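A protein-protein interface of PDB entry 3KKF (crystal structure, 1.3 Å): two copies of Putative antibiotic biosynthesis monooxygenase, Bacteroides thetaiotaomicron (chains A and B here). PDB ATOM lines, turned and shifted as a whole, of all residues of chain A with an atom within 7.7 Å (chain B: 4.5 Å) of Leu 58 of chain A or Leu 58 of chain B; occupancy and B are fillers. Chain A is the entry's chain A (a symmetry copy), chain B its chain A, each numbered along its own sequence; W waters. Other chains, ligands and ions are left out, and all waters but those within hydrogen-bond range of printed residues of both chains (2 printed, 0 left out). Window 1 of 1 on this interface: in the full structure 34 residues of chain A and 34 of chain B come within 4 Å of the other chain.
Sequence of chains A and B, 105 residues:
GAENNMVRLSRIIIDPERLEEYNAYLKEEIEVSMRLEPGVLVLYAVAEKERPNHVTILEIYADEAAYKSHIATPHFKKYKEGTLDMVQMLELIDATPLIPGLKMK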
ATOM      1  N   MET A   6       1.168 -12.145 -11.151  1.00  0.00           N
ATOM      2  CA  MET A   6       0.806 -11.233 -10.060  1.00  0.00           C
ATOM      3  C   MET A   6      -0.674 -10.973 -10.178  1.00  0.00           C
ATOM      4  O   MET A   6      -1.115 -10.444 -11.193  1.00  0.00           O
ATOM      5  CB  MET A   6       1.562  -9.937 -10.169  1.00  0.00           C
ATOM      6  CG  MET A   6       1.152  -8.915  -9.149  1.00  0.00           C
ATOM      7  SD  MET A   6       2.110  -7.243  -9.339  1.00  0.00           S
ATOM      8  CE  MET A   6       0.778  -6.124  -8.490  1.00  0.00           C
ATOM      9  N   VAL A   7      -1.431 -11.364  -9.171  1.00  0.00           N
ATOM     10  CA  VAL A   7      -2.870 -11.196  -9.119  1.00  0.00           C
ATOM     11  C   VAL A   7      -3.202 -10.236  -7.983  1.00  0.00           C
ATOM     12  O   VAL A   7      -2.694 -10.384  -6.845  1.00  0.00           O
ATOM     13  CB  VAL A   7      -3.586 -12.560  -8.919  1.00  0.00           C
ATOM     14  CG1 VAL A   7      -5.103 -12.388  -8.880  1.00  0.00           C
ATOM     15  CG2 VAL A   7      -3.190 -13.549 -10.020  1.00  0.00           C
ATOM     16  N   ARG A   8      -4.021  -9.241  -8.285  1.00  0.00           N
ATOM     17  CA  ARG A   8      -4.398  -8.255  -7.312  1.00  0.00           C
ATOM     18  C   ARG A   8      -5.820  -7.771  -7.549  1.00  0.00           C
ATOM     19  O   ARG A   8      -6.318  -7.779  -8.688  1.00  0.00           O
ATOM     20  CB  ARG A   8      -3.428  -7.055  -7.391  1.00  0.00           C
ATOM     21  CG  ARG A   8      -3.542  -6.068  -6.227  1.00  0.00           C
ATOM     22  CD  ARG A   8      -2.402  -5.042  -6.234  1.00  0.00           C
ATOM     23  NE  ARG A   8      -2.589  -4.099  -7.330  1.00  0.00           N
ATOM     24  CZ  ARG A   8      -1.769  -3.076  -7.571  1.00  0.00           C
ATOM     25  NH1 ARG A   8      -0.723  -2.861  -6.788  1.00  0.00           N
ATOM     26  NH2 ARG A   8      -2.013  -2.252  -8.591  1.00  0.00           N
ATOM     27  N   LEU A   9      -6.496  -7.404  -6.475  1.00  0.00           N
ATOM     28  CA  LEU A   9      -7.765  -6.704  -6.561  1.00  0.00           C
ATOM     29  C   LEU A   9      -7.537  -5.284  -6.124  1.00  0.00           C
ATOM     30  O   LEU A   9      -6.937  -5.033  -5.053  1.00  0.00           O
ATOM     31  CB  LEU A   9      -8.835  -7.277  -5.631  1.00  0.00           C
ATOM     32  CG  LEU A   9      -9.256  -8.692  -5.853  1.00  0.00           C
ATOM     33  CD1 LEU A   9     -10.131  -9.174  -4.701  1.00  0.00           C
ATOM     34  CD2 LEU A   9     -10.015  -8.800  -7.172  1.00  0.00           C
ATOM     35  N   SER A  10      -7.930  -4.351  -6.953  1.00  0.00           N
ATOM     36  CA  SER A  10      -7.980  -2.933  -6.554  1.00  0.00           C
ATOM     37  C   SER A  10      -9.428  -2.599  -6.260  1.00  0.00           C
ATOM     38  O   SER A  10     -10.303  -2.852  -7.095  1.00  0.00           O
ATOM     39  CB  SER A  10      -7.467  -1.988  -7.622  1.00  0.00           C
ATOM     40  OG  SER A  10      -6.098  -2.067  -7.837  1.00  0.00           O
ATOM     41  N   ARG A  11      -9.700  -2.073  -5.080  1.00  0.00           N
ATOM     42  CA  ARG A  11     -11.057  -1.624  -4.703  1.00  0.00           C
ATOM     43  C   ARG A  11     -10.970  -0.121  -4.584  1.00  0.00           C
ATOM     44  O   ARG A  11     -10.136   0.394  -3.829  1.00  0.00           O
ATOM     45  CB  ARG A  11     -11.536  -2.268  -3.403  1.00  0.00           C
ATOM     46  CG  ARG A  11     -11.932  -3.726  -3.546  1.00  0.00           C
ATOM     47  CD  ARG A  11     -12.236  -4.353  -2.223  1.00  0.00           C
ATOM     48  NE  ARG A  11     -13.148  -3.559  -1.412  1.00  0.00           N
ATOM     49  CZ  ARG A  11     -14.429  -3.852  -1.204  1.00  0.00           C
ATOM     50  NH1 ARG A  11     -14.960  -4.923  -1.749  1.00  0.00           N
ATOM     51  NH2 ARG A  11     -15.176  -3.066  -0.436  1.00  0.00           N
ATOM     52  N   ILE A  30      -7.482   1.110 -19.632  1.00  0.00           N
ATOM     53  CA  ILE A  30      -7.580  -0.366 -19.715  1.00  0.00           C
ATOM     54  C   ILE A  30      -7.499  -0.816 -21.171  1.00  0.00           C
ATOM     55  O   ILE A  30      -6.772  -1.763 -21.489  1.00  0.00           O
ATOM     56  CB  ILE A  30      -8.843  -0.882 -19.022  1.00  0.00           C
ATOM     57  CG1 ILE A  30      -8.708  -0.689 -17.503  1.00  0.00           C
ATOM     58  CG2 ILE A  30      -9.111  -2.357 -19.397  1.00  0.00           C
ATOM     59  CD1 ILE A  30      -9.923  -1.164 -16.719  1.00  0.00           C
ATOM     60  N   LEU A  41      -2.308  -9.179 -18.521  1.00  0.00           N
ATOM     61  CA  LEU A  41      -3.146 -10.311 -18.931  1.00  0.00           C
ATOM     62  C   LEU A  41      -4.628  -9.995 -18.807  1.00  0.00           C
ATOM     63  O   LEU A  41      -5.423 -10.416 -19.653  1.00  0.00           O
ATOM     64  CB  LEU A  41      -2.735 -11.602 -18.196  1.00  0.00           C
ATOM     65  CG  LEU A  41      -1.235 -11.973 -18.309  1.00  0.00           C
ATOM     66  CD1 LEU A  41      -0.949 -13.264 -17.569  1.00  0.00           C
ATOM     67  CD2 LEU A  41      -0.778 -12.088 -19.749  1.00  0.00           C
ATOM     68  N   VAL A  42      -5.012  -9.279 -17.746  1.00  0.00           N
ATOM     69  CA  VAL A  42      -6.367  -8.706 -17.694  1.00  0.00           C
ATOM     70  C   VAL A  42      -6.405  -7.566 -16.700  1.00  0.00           C
ATOM     71  O   VAL A  42      -5.694  -7.573 -15.694  1.00  0.00           O
ATOM     72  CB  VAL A  42      -7.494  -9.776 -17.344  1.00  0.00           C
ATOM     73  CG1 VAL A  42      -7.659  -9.989 -15.814  1.00  0.00           C
ATOM     74  CG2 VAL A  42      -8.838  -9.408 -18.004  1.00  0.00           C
ATOM     75  N   LEU A  43      -7.251  -6.588 -16.998  1.00  0.00           N
ATOM     76  CA  LEU A  43      -7.658  -5.520 -16.074  1.00  0.00           C
ATOM     77  C   LEU A  43      -9.186  -5.563 -16.231  1.00  0.00           C
ATOM     78  O   LEU A  43      -9.746  -4.958 -17.169  1.00  0.00           O
ATOM     79  CB  LEU A  43      -7.090  -4.153 -16.422  1.00  0.00           C
ATOM     80  CG  LEU A  43      -5.561  -4.067 -16.383  1.00  0.00           C
ATOM     81  CD1 LEU A  43      -5.021  -2.779 -17.037  1.00  0.00           C
ATOM     82  CD2 LEU A  43      -5.035  -4.216 -14.932  1.00  0.00           C
ATOM     83  N   TYR A  44      -9.864  -6.335 -15.386  1.00  0.00           N
ATOM     84  CA  TYR A  44     -11.303  -6.559 -15.482  1.00  0.00           C
ATOM     85  C   TYR A  44     -12.009  -5.735 -14.407  1.00  0.00           C
ATOM     86  O   TYR A  44     -12.079  -6.133 -13.236  1.00  0.00           O
ATOM     87  CB  TYR A  44     -11.656  -8.052 -15.383  1.00  0.00           C
ATOM     88  CG  TYR A  44     -13.085  -8.351 -15.792  1.00  0.00           C
ATOM     89  CD1 TYR A  44     -13.417  -8.639 -17.126  1.00  0.00           C
ATOM     90  CD2 TYR A  44     -14.112  -8.318 -14.870  1.00  0.00           C
ATOM     91  CE1 TYR A  44     -14.742  -8.907 -17.499  1.00  0.00           C
ATOM     92  CE2 TYR A  44     -15.429  -8.580 -15.249  1.00  0.00           C
ATOM     93  CZ  TYR A  44     -15.723  -8.875 -16.545  1.00  0.00           C
ATOM     94  OH  TYR A  44     -17.029  -9.140 -16.860  1.00  0.00           O
ATOM     95  N   ALA A  45     -12.498  -4.548 -14.803  1.00  0.00           N
ATOM     96  CA  ALA A  45     -13.147  -3.617 -13.892  1.00  0.00           C
ATOM     97  C   ALA A  45     -14.645  -3.805 -13.881  1.00  0.00           C
ATOM     98  O   ALA A  45     -15.250  -4.010 -14.923  1.00  0.00           O
ATOM     99  CB  ALA A  45     -12.793  -2.152 -14.289  1.00  0.00           C
ATOM    100  N   VAL A  46     -15.235  -3.762 -12.678  1.00  0.00           N
ATOM    101  CA  VAL A  46     -16.683  -3.807 -12.517  1.00  0.00           C
ATOM    102  C   VAL A  46     -17.112  -2.721 -11.528  1.00  0.00           C
ATOM    103  O   VAL A  46     -16.353  -2.331 -10.628  1.00  0.00           O
ATOM    104  CB  VAL A  46     -17.178  -5.185 -11.987  1.00  0.00           C
ATOM    105  CG1 VAL A  46     -16.689  -6.329 -12.884  1.00  0.00           C
ATOM    106  CG2 VAL A  46     -16.742  -5.428 -10.520  1.00  0.00           C
ATOM    107  N   VAL A  55     -15.841   0.709  -7.487  1.00  0.00           N
ATOM    108  CA  VAL A  55     -15.300  -0.074  -8.573  1.00  0.00           C
ATOM    109  C   VAL A  55     -14.252  -1.087  -8.035  1.00  0.00           C
ATOM    110  O   VAL A  55     -13.409  -0.750  -7.185  1.00  0.00           O
ATOM    111  CB  VAL A  55     -14.654   0.863  -9.639  1.00  0.00           C
ATOM    112  CG1 VAL A  55     -13.802   0.079 -10.665  1.00  0.00           C
ATOM    113  CG2 VAL A  55     -15.742   1.723 -10.320  1.00  0.00           C
ATOM    114  N   THR A  56     -14.329  -2.326  -8.504  1.00  0.00           N
ATOM    115  CA  THR A  56     -13.337  -3.346  -8.195  1.00  0.00           C
ATOM    116  C   THR A  56     -12.693  -3.771  -9.496  1.00  0.00           C
ATOM    117  O   THR A  56     -13.405  -4.010 -10.496  1.00  0.00           O
ATOM    118  CB  THR A  56     -13.966  -4.555  -7.492  1.00  0.00           C
ATOM    119  OG1 THR A  56     -14.377  -4.188  -6.193  1.00  0.00           O
ATOM    120  CG2 THR A  56     -12.956  -5.720  -7.332  1.00  0.00           C
ATOM    121  N   ILE A  57     -11.360  -3.847  -9.520  1.00  0.00           N
ATOM    122  CA  ILE A  57     -10.653  -4.303 -10.690  1.00  0.00           C
ATOM    123  C   ILE A  57      -9.860  -5.579 -10.353  1.00  0.00           C
ATOM    124  O   ILE A  57      -9.036  -5.578  -9.430  1.00  0.00           O
ATOM    125  CB  ILE A  57      -9.653  -3.229 -11.252  1.00  0.00           C
ATOM    126  CG1 ILE A  57     -10.320  -1.850 -11.361  1.00  0.00           C
ATOM    127  CG2 ILE A  57      -9.084  -3.676 -12.618  1.00  0.00           C
ATOM    128  CD1 ILE A  57      -9.434  -0.795 -11.889  1.00  0.00           C
ATOM    129  N   LEU A  58     -10.116  -6.647 -11.103  1.00  0.00           N
ATOM    130  CA  LEU A  58      -9.276  -7.847 -11.052  1.00  0.00           C
ATOM    131  C   LEU A  58      -8.125  -7.591 -12.016  1.00  0.00           C
ATOM    132  O   LEU A  58      -8.306  -7.379 -13.207  1.00  0.00           O
ATOM    133  CB  LEU A  58     -10.048  -9.091 -11.483  1.00  0.00           C
ATOM    134  CG  LEU A  58      -9.208 -10.382 -11.596  1.00  0.00           C
ATOM    135  CD1 LEU A  58      -8.534 -10.835 -10.281  1.00  0.00           C
ATOM    136  CD2 LEU A  58     -10.068 -11.508 -12.165  1.00  0.00           C
ATOM    137  N   GLU A  59      -6.932  -7.564 -11.460  1.00  0.00           N
ATOM    138  CA  GLU A  59      -5.673  -7.291 -12.196  1.00  0.00           C
ATOM    139  C   GLU A  59      -4.835  -8.531 -12.252  1.00  0.00           C
ATOM    140  O   GLU A  59      -4.558  -9.119 -11.207  1.00  0.00           O
ATOM    141  CB  GLU A  59      -4.832  -6.244 -11.460  1.00  0.00           C
ATOM    142  CG  GLU A  59      -5.527  -4.965 -11.049  1.00  0.00           C
ATOM    143  CD  GLU A  59      -4.632  -4.162 -10.074  1.00  0.00           C
ATOM    144  OE1 GLU A  59      -3.639  -3.546 -10.508  1.00  0.00           O
ATOM    145  OE2 GLU A  59      -4.933  -4.175  -8.854  1.00  0.00           O
ATOM    146  N   ILE A  60      -4.424  -8.943 -13.457  1.00  0.00           N
ATOM    147  CA  ILE A  60      -3.518 -10.089 -13.587  1.00  0.00           C
ATOM    148  C   ILE A  60      -2.373  -9.639 -14.517  1.00  0.00           C
ATOM    149  O   ILE A  60      -2.627  -9.247 -15.684  1.00  0.00           O
ATOM    150  CB  ILE A  60      -4.190 -11.366 -14.140  1.00  0.00           C
ATOM    151  CG1 ILE A  60      -5.391 -11.776 -13.284  1.00  0.00           C
ATOM    152  CG2 ILE A  60      -3.154 -12.476 -14.238  1.00  0.00           C
ATOM    153  CD1 ILE A  60      -6.221 -12.952 -13.851  1.00  0.00           C
ATOM    154  N   TYR A  61      -1.151  -9.637 -13.978  1.00  0.00           N
ATOM    155  CA  TYR A  61       0.044  -9.302 -14.721  1.00  0.00           C
ATOM    156  C   TYR A  61       0.883 -10.555 -14.868  1.00  0.00           C
ATOM    157  O   TYR A  61       0.877 -11.431 -13.999  1.00  0.00           O
ATOM    158  CB  TYR A  61       0.865  -8.211 -13.994  1.00  0.00           C
ATOM    159  CG  TYR A  61       0.067  -6.975 -13.667  1.00  0.00           C
ATOM    160  CD1 TYR A  61      -0.073  -5.965 -14.590  1.00  0.00           C
ATOM    161  CD2 TYR A  61      -0.600  -6.839 -12.447  1.00  0.00           C
ATOM    162  CE1 TYR A  61      -0.841  -4.825 -14.314  1.00  0.00           C
ATOM    163  CE2 TYR A  61      -1.345  -5.729 -12.153  1.00  0.00           C
ATOM    164  CZ  TYR A  61      -1.479  -4.721 -13.093  1.00  0.00           C
ATOM    165  OH  TYR A  61      -2.227  -3.616 -12.820  1.00  0.00           O
ATOM    166  N   ALA A  95      -3.414 -11.019  -3.923  1.00  0.00           N
ATOM    167  CA  ALA A  95      -4.245 -12.210  -3.771  1.00  0.00           C
ATOM    168  C   ALA A  95      -3.671 -13.423  -4.460  1.00  0.00           C
ATOM    169  O   ALA A  95      -2.855 -13.304  -5.391  1.00  0.00           O
ATOM    170  CB  ALA A  95      -5.658 -11.887  -4.324  1.00  0.00           C
ATOM    171  N   PRO A  97      -4.728 -16.762  -6.567  1.00  0.00           N
ATOM    172  CA  PRO A  97      -5.829 -17.438  -7.248  1.00  0.00           C
ATOM    173  C   PRO A  97      -5.943 -18.901  -6.815  1.00  0.00           C
ATOM    174  O   PRO A  97      -4.918 -19.607  -6.710  1.00  0.00           O
ATOM    175  CB  PRO A  97      -5.442 -17.332  -8.723  1.00  0.00           C
ATOM    176  CG  PRO A  97      -3.970 -17.303  -8.709  1.00  0.00           C
ATOM    177  CD  PRO A  97      -3.587 -16.533  -7.474  1.00  0.00           C
ATOM    178  N   LEU A 102      -6.661 -20.228 -14.562  1.00  0.00           N
ATOM    179  CA  LEU A 102      -8.039 -20.447 -14.987  1.00  0.00           C
ATOM    180  C   LEU A 102      -8.421 -19.239 -15.888  1.00  0.00           C
ATOM    181  O   LEU A 102      -8.140 -18.084 -15.547  1.00  0.00           O
ATOM    182  CB  LEU A 102      -8.975 -20.520 -13.780  1.00  0.00           C
ATOM    183  CG  LEU A 102     -10.432 -20.894 -14.125  1.00  0.00           C
ATOM    184  CD1 LEU A 102     -10.534 -22.354 -14.585  1.00  0.00           C
ATOM    185  CD2 LEU A 102     -11.363 -20.596 -12.949  1.00  0.00           C
ATOM    186  N   MET A 104     -11.489 -17.364 -18.612  1.00  0.00           N
ATOM    187  CA  MET A 104     -12.878 -17.202 -18.879  1.00  0.00           C
ATOM    188  C   MET A 104     -13.208 -17.923 -20.195  1.00  0.00           C
ATOM    189  O   MET A 104     -12.370 -17.922 -21.140  1.00  0.00           O
ATOM    190  CB  MET A 104     -13.170 -15.713 -19.057  1.00  0.00           C
ATOM    191  CG  MET A 104     -12.790 -14.800 -17.857  1.00  0.00           C
ATOM    192  SD  MET A 104     -13.001 -12.964 -18.287  1.00  0.00           S
ATOM    193  CE  MET A 104     -12.640 -12.181 -16.553  1.00  0.00           C
ATOM    194  N   VAL B   7     -22.847 -10.782 -14.087  1.00  0.00           N
ATOM    195  CA  VAL B   7     -21.557 -10.608 -13.449  1.00  0.00           C
ATOM    196  C   VAL B   7     -21.787 -10.272 -11.980  1.00  0.00           C
ATOM    197  O   VAL B   7     -22.613  -9.390 -11.643  1.00  0.00           O
ATOM    198  CB  VAL B   7     -20.733  -9.492 -14.148  1.00  0.00           C
ATOM    199  CG1 VAL B   7     -19.367  -9.316 -13.488  1.00  0.00           C
ATOM    200  CG2 VAL B   7     -20.568  -9.792 -15.642  1.00  0.00           C
ATOM    201  N   ARG B   8     -21.092 -10.983 -11.106  1.00  0.00           N
ATOM    202  CA  ARG B   8     -21.231 -10.781  -9.692  1.00  0.00           C
ATOM    203  C   ARG B   8     -19.913 -11.027  -8.975  1.00  0.00           C
ATOM    204  O   ARG B   8     -19.069 -11.815  -9.435  1.00  0.00           O
ATOM    205  CB  ARG B   8     -22.303 -11.745  -9.136  1.00  0.00           C
ATOM    206  CG  ARG B   8     -22.750 -11.441  -7.705  1.00  0.00           C
ATOM    207  CD  ARG B   8     -23.976 -12.270  -7.301  1.00  0.00           C
ATOM    208  NE  ARG B   8     -23.594 -13.664  -7.111  1.00  0.00           N
ATOM    209  CZ  ARG B   8     -24.444 -14.618  -6.731  1.00  0.00           C
ATOM    210  NH1 ARG B   8     -25.712 -14.322  -6.488  1.00  0.00           N
ATOM    211  NH2 ARG B   8     -24.013 -15.869  -6.572  1.00  0.00           N
ATOM    212  N   LEU B   9     -19.705 -10.316  -7.881  1.00  0.00           N
ATOM    213  CA  LEU B   9     -18.614 -10.603  -6.965  1.00  0.00           C
ATOM    214  C   LEU B   9     -19.208 -11.183  -5.713  1.00  0.00           C
ATOM    215  O   LEU B   9     -20.164 -10.615  -5.135  1.00  0.00           O
ATOM    216  CB  LEU B   9     -17.837  -9.357  -6.542  1.00  0.00           C
ATOM    217  CG  LEU B   9     -17.138  -8.584  -7.610  1.00  0.00           C
ATOM    218  CD1 LEU B   9     -16.630  -7.255  -7.060  1.00  0.00           C
ATOM    219  CD2 LEU B   9     -15.975  -9.404  -8.158  1.00  0.00           C
ATOM    220  N   VAL B  42     -17.008 -18.066 -15.967  1.00  0.00           N
ATOM    221  CA  VAL B  42     -15.862 -18.155 -15.047  1.00  0.00           C
ATOM    222  C   VAL B  42     -16.348 -18.090 -13.615  1.00  0.00           C
ATOM    223  O   VAL B  42     -17.342 -17.430 -13.310  1.00  0.00           O
ATOM    224  CB  VAL B  42     -14.756 -17.038 -15.302  1.00  0.00           C
ATOM    225  CG1 VAL B  42     -15.079 -15.703 -14.575  1.00  0.00           C
ATOM    226  CG2 VAL B  42     -13.349 -17.549 -14.930  1.00  0.00           C
ATOM    227  N   LEU B  43     -15.626 -18.782 -12.743  1.00  0.00           N
ATOM    228  CA  LEU B  43     -15.734 -18.665 -11.283  1.00  0.00           C
ATOM    229  C   LEU B  43     -14.256 -18.505 -10.892  1.00  0.00           C
ATOM    230  O   LEU B  43     -13.524 -19.506 -10.752  1.00  0.00           O
ATOM    231  CB  LEU B  43     -16.372 -19.871 -10.612  1.00  0.00           C
ATOM    232  CG  LEU B  43     -17.818 -20.148 -11.034  1.00  0.00           C
ATOM    233  CD1 LEU B  43     -18.315 -21.537 -10.582  1.00  0.00           C
ATOM    234  CD2 LEU B  43     -18.766 -19.029 -10.534  1.00  0.00           C
ATOM    235  N   TYR B  44     -13.782 -17.266 -10.796  1.00  0.00           N
ATOM    236  CA  TYR B  44     -12.378 -16.962 -10.542  1.00  0.00           C
ATOM    237  C   TYR B  44     -12.218 -16.528  -9.086  1.00  0.00           C
ATOM    238  O   TYR B  44     -12.478 -15.370  -8.729  1.00  0.00           O
ATOM    239  CB  TYR B  44     -11.835 -15.905 -11.517  1.00  0.00           C
ATOM    240  CG  TYR B  44     -10.323 -15.798 -11.492  1.00  0.00           C
ATOM    241  CD1 TYR B  44      -9.522 -16.590 -12.331  1.00  0.00           C
ATOM    242  CD2 TYR B  44      -9.683 -14.938 -10.621  1.00  0.00           C
ATOM    243  CE1 TYR B  44      -8.123 -16.492 -12.298  1.00  0.00           C
ATOM    244  CE2 TYR B  44      -8.292 -14.849 -10.590  1.00  0.00           C
ATOM    245  CZ  TYR B  44      -7.536 -15.614 -11.425  1.00  0.00           C
ATOM    246  OH  TYR B  44      -6.176 -15.476 -11.365  1.00  0.00           O
ATOM    247  N   THR B  56     -12.602 -13.711  -2.470  1.00  0.00           N
ATOM    248  CA  THR B  56     -13.457 -13.010  -3.415  1.00  0.00           C
ATOM    249  C   THR B  56     -13.550 -13.853  -4.668  1.00  0.00           C
ATOM    250  O   THR B  56     -12.515 -14.356  -5.160  1.00  0.00           O
ATOM    251  CB  THR B  56     -12.907 -11.617  -3.752  1.00  0.00           C
ATOM    252  OG1 THR B  56     -13.020 -10.777  -2.623  1.00  0.00           O
ATOM    253  CG2 THR B  56     -13.704 -10.942  -4.897  1.00  0.00           C
ATOM    254  N   ILE B  57     -14.766 -14.046  -5.184  1.00  0.00           N
ATOM    255  CA  ILE B  57     -14.954 -14.780  -6.409  1.00  0.00           C
ATOM    256  C   ILE B  57     -15.592 -13.866  -7.471  1.00  0.00           C
ATOM    257  O   ILE B  57     -16.665 -13.294  -7.242  1.00  0.00           O
ATOM    258  CB  ILE B  57     -15.873 -16.042  -6.225  1.00  0.00           C
ATOM    259  CG1 ILE B  57     -15.447 -16.868  -5.001  1.00  0.00           C
ATOM    260  CG2 ILE B  57     -15.871 -16.910  -7.503  1.00  0.00           C
ATOM    261  CD1 ILE B  57     -16.268 -18.073  -4.775  1.00  0.00           C
ATOM    262  N   LEU B  58     -14.926 -13.739  -8.615  1.00  0.00           N
ATOM    263  CA  LEU B  58     -15.523 -13.098  -9.790  1.00  0.00           C
ATOM    264  C   LEU B  58     -16.312 -14.189 -10.505  1.00  0.00           C
ATOM    265  O   LEU B  58     -15.782 -15.206 -10.930  1.00  0.00           O
ATOM    266  CB  LEU B  58     -14.457 -12.533 -10.724  1.00  0.00           C
ATOM    267  CG  LEU B  58     -14.984 -11.961 -12.059  1.00  0.00           C
ATOM    268  CD1 LEU B  58     -15.973 -10.783 -11.914  1.00  0.00           C
ATOM    269  CD2 LEU B  58     -13.809 -11.560 -12.947  1.00  0.00           C
ATOM    270  N   GLU B  59     -17.610 -13.976 -10.577  1.00  0.00           N
ATOM    271  CA  GLU B  59     -18.577 -14.919 -11.190  1.00  0.00           C
ATOM    272  C   GLU B  59     -19.130 -14.335 -12.454  1.00  0.00           C
ATOM    273  O   GLU B  59     -19.638 -13.215 -12.429  1.00  0.00           O
ATOM    274  CB  GLU B  59     -19.777 -15.140 -10.264  1.00  0.00           C
ATOM    275  CG  GLU B  59     -19.481 -15.499  -8.826  1.00  0.00           C
ATOM    276  CD  GLU B  59     -20.771 -15.395  -7.975  1.00  0.00           C
ATOM    277  OE1 GLU B  59     -21.650 -16.274  -8.071  1.00  0.00           O
ATOM    278  OE2 GLU B  59     -20.897 -14.398  -7.218  1.00  0.00           O
ATOM    279  N   ILE B  60     -19.040 -15.075 -13.566  1.00  0.00           N
ATOM    280  CA  ILE B  60     -19.648 -14.618 -14.820  1.00  0.00           C
ATOM    281  C   ILE B  60     -20.474 -15.800 -15.364  1.00  0.00           C
ATOM    282  O   ILE B  60     -19.914 -16.897 -15.614  1.00  0.00           O
ATOM    283  CB  ILE B  60     -18.628 -14.142 -15.878  1.00  0.00           C
ATOM    284  CG1 ILE B  60     -17.731 -13.031 -15.325  1.00  0.00           C
ATOM    285  CG2 ILE B  60     -19.372 -13.704 -17.131  1.00  0.00           C
ATOM    286  CD1 ILE B  60     -16.576 -12.603 -16.262  1.00  0.00           C
ATOM    287  N   MET B 104      -9.365 -12.661 -20.491  1.00  0.00           N
ATOM    288  CA  MET B 104      -8.014 -12.736 -20.049  1.00  0.00           C
ATOM    289  C   MET B 104      -7.150 -13.247 -21.211  1.00  0.00           C
ATOM    290  O   MET B 104      -7.611 -14.113 -22.006  1.00  0.00           O
ATOM    291  CB  MET B 104      -7.931 -13.744 -18.905  1.00  0.00           C
ATOM    292  CG  MET B 104      -8.836 -13.449 -17.673  1.00  0.00           C
ATOM    293  SD  MET B 104      -8.801 -14.879 -16.428  1.00  0.00           S
ATOM    294  CE  MET B 104      -9.846 -14.090 -15.000  1.00  0.00           C
HETATM  295  O   HOH W   1      -5.654 -16.639 -15.631  1.00  0.00           O
HETATM  296  O   HOH W   2     -10.143 -15.673 -20.879  1.00  0.00           O
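O of Leu 102 of chain A lies close to SD of Met 104 of chain B (3.4 Å).
The backbone carbonyl oxygen (O) of Val 42 of chain A lies within hydrogen-bond range of the backbone NH (N) of Ile 60 of chain A, at 2.9 Å. The backbone NH (N) of Ile 60 of chain B sits at hydrogen-bond distance from the backbone carbonyl oxygen (O) of Val 42 of chain B (2.9 Å). The backbone NH (N) of Tyr 44 of chain B lies within hydrogen-bond range of the backbone carbonyl oxygen (O) of Leu 58 of chain B, at 2.9 Å. The backbone carbonyl oxygen of Thr 56 of chain A is in hydrogen-bond range of the backbone NH of Val 46 of chain A, at 2.9 Å. O of Ile 60 of chain A sits at hydrogen-bond distance from N of Leu 41 of chain A.
Among the printed residues, pairs that only touch across the chains: Val 7 of chain A with Tyr 44 of chain B, Leu 9 of chain A with Thr 56 of chain B, Leu 41 of chain A with Met 104 of chain B, Val 42 of chain A with Met 104 of chain B, Tyr 44 of chain A with Val 7 of chain B, Tyr 44 of chain A with Leu 58 of chain B, Tyr 44 of chain A with Ile 60 of chain B, Val 46 of chain A with Leu 9 of chain B, Thr 56 of chain A with Leu 9 of chain B, Leu 58 of chain A with Tyr 44 of chain B, Leu 58 of chain A with Leu 58 of chain B, Leu 58 of chain A with Met 104 of chain B, Ile 60 of chain A with Tyr 44 of chain B, Ile 60 of chain A with Met 104 of chain B, Pro 97 of chain A with Tyr 44 of chain B, Leu 102 of chain A with Leu 43 of chain B, Leu 102 of chain A with Tyr 44 of chain B, Met 104 of chain A with Val 42 of chain B, Met 104 of chain A with Leu 58 of chain B, Met 104 of chain A with Ile 60 of chain B and Met 104 of chain A with Met 104 of chain B.
Printed residues of chain B within 4 Å of Val 46 of chain A: Leu 9. Of the printed residues of chain B, Leu 58 of chain A touches Tyr 44 (3.8 Å), Leu 58 (3.8 Å) and Met 104 (3.8 Å). Of the printed residues of chain B, Leu 102 of chain A touches Leu 43 (3.3 Å), Tyr 44 (3.6 Å) and Met 104 (3.4 Å). Ile 57 of chain B touches none of the printed residues of chain A. Of the printed residues of chain A, Leu 58 of chain B touches Tyr 44 (3.8 Å), Leu 58 (3.8 Å) and Met 104 (3.8 Å). The nearest printed residue of chain B that does not touch Leu 58 of chain A is Leu 9 of chain B (6.8 Å). The nearest printed residue of chain A that does not touch Leu 58 of chain B is Val 46 of chain A (4.6 Å).
Hydrophobic or aromatic side chains of chain A that line the printed part of chain B: Val 7, Leu 9, Val 42, Tyr 44, Val 46, Leu 58, Ile 60, Pro 97, Leu 102 and Met 104. Along chain A the printed residues that touch a printed residue of chain B span positions 7 to 104. Hydrophobic or aromatic side chains of chain B within 4 Å of the printed part of chain A: Val 7, Leu 9, Val 42, Tyr 44, Leu 58, Ile 60 and Met 104. Among the printed residues, 22 pairs touch across the chains.
Leu 9 of chain A touches Thr 56 of chain B, and with the chains exchanged Thr 56 of chain A touches Leu 9 of chain B. Tyr 44 of chain A touches Ile 60 of chain B, and with the chains exchanged Ile 60 of chain A touches Tyr 44 of chain B. Ile 60 of chain A touches Met 104 of chain B, and with the chains exchanged Met 104 of chain A touches Ile 60 of chain B. Met 104 of chain A touches its own counterpart, Met 104 of chain B. Positions printed for both chains: 7, 8, 9, 42, 43, 44, 56, 57, 58, 59, 60 and 104. Of the 22 pairs that touch across the chains among the printed residues, 16 have their exchanged pair printed and touching as well.
Water W1 bridges O of Leu 102 of chain A and SD of Met 104 of chain B. Water W2 bridges the backbone NH of Met 104 of chain A (3.1 Å) and the backbone NH of Met 104 of chain B (3.1 Å).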
